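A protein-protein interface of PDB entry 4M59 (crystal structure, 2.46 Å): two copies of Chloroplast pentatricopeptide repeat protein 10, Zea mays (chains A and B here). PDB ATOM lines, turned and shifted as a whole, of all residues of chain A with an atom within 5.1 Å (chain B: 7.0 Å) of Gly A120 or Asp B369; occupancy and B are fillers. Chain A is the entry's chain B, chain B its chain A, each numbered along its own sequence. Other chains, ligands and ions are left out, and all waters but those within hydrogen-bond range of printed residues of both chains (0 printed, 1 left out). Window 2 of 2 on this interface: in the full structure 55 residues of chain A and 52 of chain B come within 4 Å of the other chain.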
ATOM      1  N   LEU A 116     -22.814 -29.165 -10.840  1.00  0.00           N
ATOM      2  CA  LEU A 116     -22.763 -29.311 -12.266  1.00  0.00           C
ATOM      3  C   LEU A 116     -24.091 -28.906 -12.859  1.00  0.00           C
ATOM      4  O   LEU A 116     -24.144 -28.268 -13.897  1.00  0.00           O
ATOM      5  CB  LEU A 116     -22.475 -30.757 -12.612  1.00  0.00           C
ATOM      6  CG  LEU A 116     -21.204 -31.309 -12.012  1.00  0.00           C
ATOM      7  CD1 LEU A 116     -21.252 -32.785 -12.073  1.00  0.00           C
ATOM      8  CD2 LEU A 116     -20.047 -30.806 -12.782  1.00  0.00           C
ATOM      9  N   SER A 117     -25.162 -29.297 -12.196  1.00  0.00           N
ATOM     10  CA  SER A 117     -26.499 -28.951 -12.619  1.00  0.00           C
ATOM     11  C   SER A 117     -26.602 -27.450 -12.669  1.00  0.00           C
ATOM     12  O   SER A 117     -27.072 -26.865 -13.633  1.00  0.00           O
ATOM     13  CB  SER A 117     -27.513 -29.515 -11.631  1.00  0.00           C
ATOM     14  OG  SER A 117     -28.842 -29.167 -11.960  1.00  0.00           O
ATOM     15  N   ARG A 118     -26.110 -26.827 -11.619  1.00  0.00           N
ATOM     16  CA  ARG A 118     -26.130 -25.392 -11.465  1.00  0.00           C
ATOM     17  C   ARG A 118     -25.311 -24.700 -12.550  1.00  0.00           C
ATOM     18  O   ARG A 118     -25.336 -23.488 -12.673  1.00  0.00           O
ATOM     19  CB  ARG A 118     -25.556 -25.079 -10.097  1.00  0.00           C
ATOM     20  CG  ARG A 118     -25.857 -23.724  -9.564  1.00  0.00           C
ATOM     21  CD  ARG A 118     -27.176 -23.666  -8.846  1.00  0.00           C
ATOM     22  NE  ARG A 118     -28.007 -22.632  -9.429  1.00  0.00           N
ATOM     23  CZ  ARG A 118     -27.807 -21.336  -9.264  1.00  0.00           C
ATOM     24  NH1 ARG A 118     -26.811 -20.906  -8.519  1.00  0.00           N
ATOM     25  NH2 ARG A 118     -28.608 -20.469  -9.849  1.00  0.00           N
ATOM     26  N   ALA A 119     -24.601 -25.478 -13.348  1.00  0.00           N
ATOM     27  CA  ALA A 119     -23.750 -24.933 -14.384  1.00  0.00           C
ATOM     28  C   ALA A 119     -24.187 -25.392 -15.745  1.00  0.00           C
ATOM     29  O   ALA A 119     -23.582 -25.047 -16.742  1.00  0.00           O
ATOM     30  CB  ALA A 119     -22.345 -25.351 -14.152  1.00  0.00           C
ATOM     31  N   GLY A 120     -25.231 -26.202 -15.777  1.00  0.00           N
ATOM     32  CA  GLY A 120     -25.754 -26.709 -17.019  1.00  0.00           C
ATOM     33  C   GLY A 120     -24.945 -27.856 -17.536  1.00  0.00           C
ATOM     34  O   GLY A 120     -25.025 -28.208 -18.694  1.00  0.00           O
ATOM     35  N   ARG A 121     -24.158 -28.448 -16.671  1.00  0.00           N
ATOM     36  CA  ARG A 121     -23.369 -29.582 -17.065  1.00  0.00           C
ATOM     37  C   ARG A 121     -24.107 -30.851 -16.741  1.00  0.00           C
ATOM     38  O   ARG A 121     -23.678 -31.639 -15.922  1.00  0.00           O
ATOM     39  CB  ARG A 121     -22.014 -29.552 -16.379  1.00  0.00           C
ATOM     40  CG  ARG A 121     -21.169 -28.379 -16.799  1.00  0.00           C
ATOM     41  CD  ARG A 121     -19.868 -28.342 -16.067  1.00  0.00           C
ATOM     42  NE  ARG A 121     -19.008 -29.461 -16.409  1.00  0.00           N
ATOM     43  CZ  ARG A 121     -17.812 -29.653 -15.885  1.00  0.00           C
ATOM     44  NH1 ARG A 121     -17.344 -28.803 -14.998  1.00  0.00           N
ATOM     45  NH2 ARG A 121     -17.092 -30.696 -16.241  1.00  0.00           N
ATOM     46  N   TYR A 122     -25.231 -31.040 -17.408  1.00  0.00           N
ATOM     47  CA  TYR A 122     -26.096 -32.157 -17.133  1.00  0.00           C
ATOM     48  C   TYR A 122     -25.447 -33.462 -17.535  1.00  0.00           C
ATOM     49  O   TYR A 122     -25.712 -34.499 -16.960  1.00  0.00           O
ATOM     50  CB  TYR A 122     -27.400 -31.990 -17.885  1.00  0.00           C
ATOM     51  CG  TYR A 122     -27.999 -30.626 -17.780  1.00  0.00           C
ATOM     52  CD1 TYR A 122     -28.470 -30.154 -16.582  1.00  0.00           C
ATOM     53  CD2 TYR A 122     -28.108 -29.813 -18.882  1.00  0.00           C
ATOM     54  CE1 TYR A 122     -29.017 -28.915 -16.476  1.00  0.00           C
ATOM     55  CE2 TYR A 122     -28.658 -28.574 -18.789  1.00  0.00           C
ATOM     56  CZ  TYR A 122     -29.112 -28.127 -17.577  1.00  0.00           C
ATOM     57  OH  TYR A 122     -29.660 -26.880 -17.471  1.00  0.00           O
ATOM     58  N   LEU B 337     -29.415 -22.516 -29.590  1.00  0.00           N
ATOM     59  CA  LEU B 337     -28.406 -23.398 -30.142  1.00  0.00           C
ATOM     60  C   LEU B 337     -28.896 -24.177 -31.339  1.00  0.00           C
ATOM     61  O   LEU B 337     -28.170 -24.336 -32.302  1.00  0.00           O
ATOM     62  CB  LEU B 337     -27.914 -24.359 -29.073  1.00  0.00           C
ATOM     63  CG  LEU B 337     -27.062 -23.732 -27.992  1.00  0.00           C
ATOM     64  CD1 LEU B 337     -26.691 -24.767 -26.999  1.00  0.00           C
ATOM     65  CD2 LEU B 337     -25.841 -23.177 -28.620  1.00  0.00           C
ATOM     66  N   ARG B 365     -29.659 -20.102 -15.002  1.00  0.00           N
ATOM     67  CA  ARG B 365     -29.130 -21.411 -14.639  1.00  0.00           C
ATOM     68  C   ARG B 365     -28.719 -22.196 -15.878  1.00  0.00           C
ATOM     69  O   ARG B 365     -29.464 -22.268 -16.850  1.00  0.00           O
ATOM     70  CB  ARG B 365     -30.168 -22.199 -13.845  1.00  0.00           C
ATOM     71  CG  ARG B 365     -29.579 -23.243 -12.910  1.00  0.00           C
ATOM     72  CD  ARG B 365     -30.432 -24.495 -12.885  1.00  0.00           C
ATOM     73  NE  ARG B 365     -31.211 -24.602 -11.656  1.00  0.00           N
ATOM     74  CZ  ARG B 365     -31.090 -25.591 -10.779  1.00  0.00           C
ATOM     75  NH1 ARG B 365     -30.218 -26.565 -10.996  1.00  0.00           N
ATOM     76  NH2 ARG B 365     -31.841 -25.607  -9.687  1.00  0.00           N
ATOM     77  N   GLY B 366     -27.528 -22.789 -15.830  1.00  0.00           N
ATOM     78  CA  GLY B 366     -27.027 -23.582 -16.933  1.00  0.00           C
ATOM     79  C   GLY B 366     -26.477 -22.741 -18.068  1.00  0.00           C
ATOM     80  O   GLY B 366     -26.329 -23.219 -19.191  1.00  0.00           O
ATOM     81  N   MET B 367     -26.167 -21.484 -17.769  1.00  0.00           N
ATOM     82  CA  MET B 367     -25.644 -20.568 -18.776  1.00  0.00           C
ATOM     83  C   MET B 367     -24.189 -20.871 -19.110  1.00  0.00           C
ATOM     84  O   MET B 367     -23.743 -20.653 -20.234  1.00  0.00           O
ATOM     85  CB  MET B 367     -25.781 -19.122 -18.299  1.00  0.00           C
ATOM     86  CG  MET B 367     -24.963 -18.124 -19.104  1.00  0.00           C
ATOM     87  SD  MET B 367     -25.288 -16.413 -18.649  1.00  0.00           S
ATOM     88  CE  MET B 367     -24.049 -15.565 -19.622  1.00  0.00           C
ATOM     89  N   GLU B 368     -23.452 -21.376 -18.127  1.00  0.00           N
ATOM     90  CA  GLU B 368     -22.037 -21.673 -18.308  1.00  0.00           C
ATOM     91  C   GLU B 368     -21.799 -22.696 -19.414  1.00  0.00           C
ATOM     92  O   GLU B 368     -20.850 -22.572 -20.187  1.00  0.00           O
ATOM     93  CB  GLU B 368     -21.423 -22.166 -17.000  1.00  0.00           C
ATOM     94  CG  GLU B 368     -20.029 -22.751 -17.159  1.00  0.00           C
ATOM     95  CD  GLU B 368     -19.490 -23.328 -15.866  1.00  0.00           C
ATOM     96  OE1 GLU B 368     -18.401 -23.936 -15.897  1.00  0.00           O
ATOM     97  OE2 GLU B 368     -20.151 -23.173 -14.820  1.00  0.00           O
ATOM     98  N   ASP B 369     -22.657 -23.706 -19.484  1.00  0.00           N
ATOM     99  CA  ASP B 369     -22.507 -24.747 -20.471  1.00  0.00           C
ATOM    100  C   ASP B 369     -22.905 -24.228 -21.817  1.00  0.00           C
ATOM    101  O   ASP B 369     -22.379 -24.644 -22.833  1.00  0.00           O
ATOM    102  CB  ASP B 369     -23.377 -25.930 -20.104  1.00  0.00           C
ATOM    103  CG  ASP B 369     -23.097 -27.119 -20.941  1.00  0.00           C
ATOM    104  OD1 ASP B 369     -21.923 -27.371 -21.221  1.00  0.00           O
ATOM    105  OD2 ASP B 369     -24.053 -27.802 -21.330  1.00  0.00           O
ATOM    106  N   TYR B 370     -23.845 -23.303 -21.818  1.00  0.00           N
ATOM    107  CA  TYR B 370     -24.295 -22.682 -23.037  1.00  0.00           C
ATOM    108  C   TYR B 370     -23.153 -21.942 -23.673  1.00  0.00           C
ATOM    109  O   TYR B 370     -22.821 -22.176 -24.814  1.00  0.00           O
ATOM    110  CB  TYR B 370     -25.443 -21.743 -22.726  1.00  0.00           C
ATOM    111  CG  TYR B 370     -25.787 -20.743 -23.796  1.00  0.00           C
ATOM    112  CD1 TYR B 370     -26.583 -21.076 -24.864  1.00  0.00           C
ATOM    113  CD2 TYR B 370     -25.348 -19.451 -23.703  1.00  0.00           C
ATOM    114  CE1 TYR B 370     -26.900 -20.153 -25.809  1.00  0.00           C
ATOM    115  CE2 TYR B 370     -25.664 -18.536 -24.645  1.00  0.00           C
ATOM    116  CZ  TYR B 370     -26.435 -18.884 -25.688  1.00  0.00           C
ATOM    117  OH  TYR B 370     -26.727 -17.936 -26.611  1.00  0.00           O
ATOM    118  N   VAL B 371     -22.535 -21.062 -22.906  1.00  0.00           N
ATOM    119  CA  VAL B 371     -21.415 -20.284 -23.382  1.00  0.00           C
ATOM    120  C   VAL B 371     -20.298 -21.168 -23.875  1.00  0.00           C
ATOM    121  O   VAL B 371     -19.638 -20.863 -24.849  1.00  0.00           O
ATOM    122  CB  VAL B 371     -20.884 -19.398 -22.272  1.00  0.00           C
ATOM    123  CG1 VAL B 371     -19.770 -18.531 -22.781  1.00  0.00           C
ATOM    124  CG2 VAL B 371     -21.986 -18.544 -21.738  1.00  0.00           C
ATOM    125  N   THR B 372     -20.093 -22.279 -23.199  1.00  0.00           N
ATOM    126  CA  THR B 372     -19.092 -23.219 -23.627  1.00  0.00           C
ATOM    127  C   THR B 372     -19.517 -23.810 -24.942  1.00  0.00           C
ATOM    128  O   THR B 372     -18.702 -24.051 -25.810  1.00  0.00           O
ATOM    129  CB  THR B 372     -18.917 -24.318 -22.604  1.00  0.00           C
ATOM    130  OG1 THR B 372     -18.626 -23.739 -21.334  1.00  0.00           O
ATOM    131  CG2 THR B 372     -17.778 -25.194 -22.989  1.00  0.00           C
ATOM    132  N   ARG B 373     -20.813 -24.027 -25.098  1.00  0.00           N
ATOM    133  CA  ARG B 373     -21.325 -24.645 -26.304  1.00  0.00           C
ATOM    134  C   ARG B 373     -21.296 -23.691 -27.473  1.00  0.00           C
ATOM    135  O   ARG B 373     -21.272 -24.112 -28.613  1.00  0.00           O
ATOM    136  CB  ARG B 373     -22.736 -25.164 -26.076  1.00  0.00           C
ATOM    137  CG  ARG B 373     -23.032 -26.432 -26.812  1.00  0.00           C
ATOM    138  CD  ARG B 373     -22.021 -27.498 -26.461  1.00  0.00           C
ATOM    139  NE  ARG B 373     -22.196 -28.067 -25.130  1.00  0.00           N
ATOM    140  CZ  ARG B 373     -21.197 -28.484 -24.360  1.00  0.00           C
ATOM    141  NH1 ARG B 373     -19.945 -28.378 -24.769  1.00  0.00           N
ATOM    142  NH2 ARG B 373     -21.445 -28.993 -23.173  1.00  0.00           N
ATOM    143  N   VAL B 374     -21.299 -22.401 -27.179  1.00  0.00           N
ATOM    144  CA  VAL B 374     -21.207 -21.369 -28.190  1.00  0.00           C
ATOM    145  C   VAL B 374     -19.775 -21.173 -28.591  1.00  0.00           C
ATOM    146  O   VAL B 374     -19.443 -21.120 -29.762  1.00  0.00           O
ATOM    147  CB  VAL B 374     -21.704 -20.040 -27.649  1.00  0.00           C
ATOM    148  CG1 VAL B 374     -21.404 -18.948 -28.611  1.00  0.00           C
ATOM    149  CG2 VAL B 374     -23.167 -20.095 -27.389  1.00  0.00           C
ATOM    150  N   LEU B 375     -18.921 -21.072 -27.594  1.00  0.00           N
ATOM    151  CA  LEU B 375     -17.503 -20.920 -27.792  1.00  0.00           C
ATOM    152  C   LEU B 375     -16.930 -22.104 -28.544  1.00  0.00           C
ATOM    153  O   LEU B 375     -15.993 -21.976 -29.303  1.00  0.00           O
ATOM    154  CB  LEU B 375     -16.857 -20.788 -26.433  1.00  0.00           C
ATOM    155  CG  LEU B 375     -15.352 -20.730 -26.281  1.00  0.00           C
ATOM    156  CD1 LEU B 375     -14.776 -19.719 -27.200  1.00  0.00           C
ATOM    157  CD2 LEU B 375     -15.083 -20.349 -24.864  1.00  0.00           C
ATOM    158  N   TYR B 397     -18.756 -15.685 -19.122  1.00  0.00           N
ATOM    159  CA  TYR B 397     -18.291 -16.678 -18.164  1.00  0.00           C
ATOM    160  C   TYR B 397     -18.226 -16.049 -16.778  1.00  0.00           C
ATOM    161  O   TYR B 397     -18.349 -16.738 -15.766  1.00  0.00           O
ATOM    162  CB  TYR B 397     -16.917 -17.215 -18.571  1.00  0.00           C
ATOM    163  CG  TYR B 397     -16.974 -18.490 -19.379  1.00  0.00           C
ATOM    164  CD1 TYR B 397     -18.025 -19.385 -19.232  1.00  0.00           C
ATOM    165  CD2 TYR B 397     -15.977 -18.798 -20.293  1.00  0.00           C
ATOM    166  CE1 TYR B 397     -18.080 -20.550 -19.969  1.00  0.00           C
ATOM    167  CE2 TYR B 397     -16.022 -19.963 -21.036  1.00  0.00           C
ATOM    168  CZ  TYR B 397     -17.076 -20.835 -20.870  1.00  0.00           C
ATOM    169  OH  TYR B 397     -17.126 -21.997 -21.607  1.00  0.00           O
ATOM    170  N   CYS B 400     -22.104 -15.628 -15.494  1.00  0.00           N
ATOM    171  CA  CYS B 400     -22.714 -16.814 -14.954  1.00  0.00           C
ATOM    172  C   CYS B 400     -21.983 -17.243 -13.714  1.00  0.00           C
ATOM    173  O   CYS B 400     -22.506 -17.922 -12.875  1.00  0.00           O
ATOM    174  CB  CYS B 400     -22.730 -17.929 -15.982  1.00  0.00           C
ATOM    175  SG  CYS B 400     -21.279 -18.239 -16.848  1.00  0.00           S
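The backbone carbonyl oxygen of Ala A119 is in hydrogen-bond range of the backbone NH of Asp B369.
The side-chain carboxylate (OD2) of Asp B369 lies close to the backbone carbonyl oxygen (O) of Gly A120 (2.8 Å).
The guanidinium group (NH1) of Arg B365 is in hydrogen-bond range of the side-chain hydroxyl (OG) of Ser A117.
The backbone carbonyl oxygen (O) of Glu B368 lies within hydrogen-bond range of the side-chain hydroxyl (OG1) of Thr B372 (2.8 Å).
The side-chain carboxylate (OD1) of Asp B369 is in salt-bridge range of the guanidinium group (NH2) of Arg B373 (2.6 Å).
Arg A118 touches Arg B365 (NE to CG, 3.9 Å).
Arg A118 touches Gly B366.
Gly B366 touches Ala A119 (CA to C, 3.6 Å).
Ala A119 touches Glu B368.
Gly A120 touches Gly B366 (CA to CA, 3.4 Å).
Printed residues of chain B within 4 Å of Arg A118: Arg B365 (3.9 Å) and Gly B366 (3.9 Å).
Gly A120 touches two residues of chain B.
Of the printed residues of chain A, Arg B365 touches Ser A117 and Arg A118.
Of the printed residues of chain A, Gly B366 touches Arg A118 (3.9 Å), Ala A119 (3.6 Å) and Gly A120 (3.4 Å).
Met B367 touches none of the printed residues of chain A.
Printed residues of chain A within 4 Å of Glu B368: Ala A119.
Asp B369 touches just these residues of chain A: Ala A119 (3.2 Å) and Gly A120 (2.8 Å).
Leu B375 touches none of the printed residues of chain A.
The nearest residue of chain B that does not touch Gly A120 is Met B367 (5.2 Å).
The nearest printed residue of chain B that does not touch Ala A119 is Met B367 (4.5 Å).
Hydrophobic or aromatic side chains of chain A that line the printed part of chain B: Ala A119.
Of the 14 printed residues of chain B, 4 touch a printed residue of chain A.
Among the printed residues, 8 pairs touch across the chains.
Among the printed residues, no Asp or Glu carboxylate lies within 4 Å of a Lys or Arg side-chain nitrogen of the other chain.
No position is printed for both chains.
Of the 8 pairs that touch across the chains among the printed residues, none has its exchanged pair printed and touching as well.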
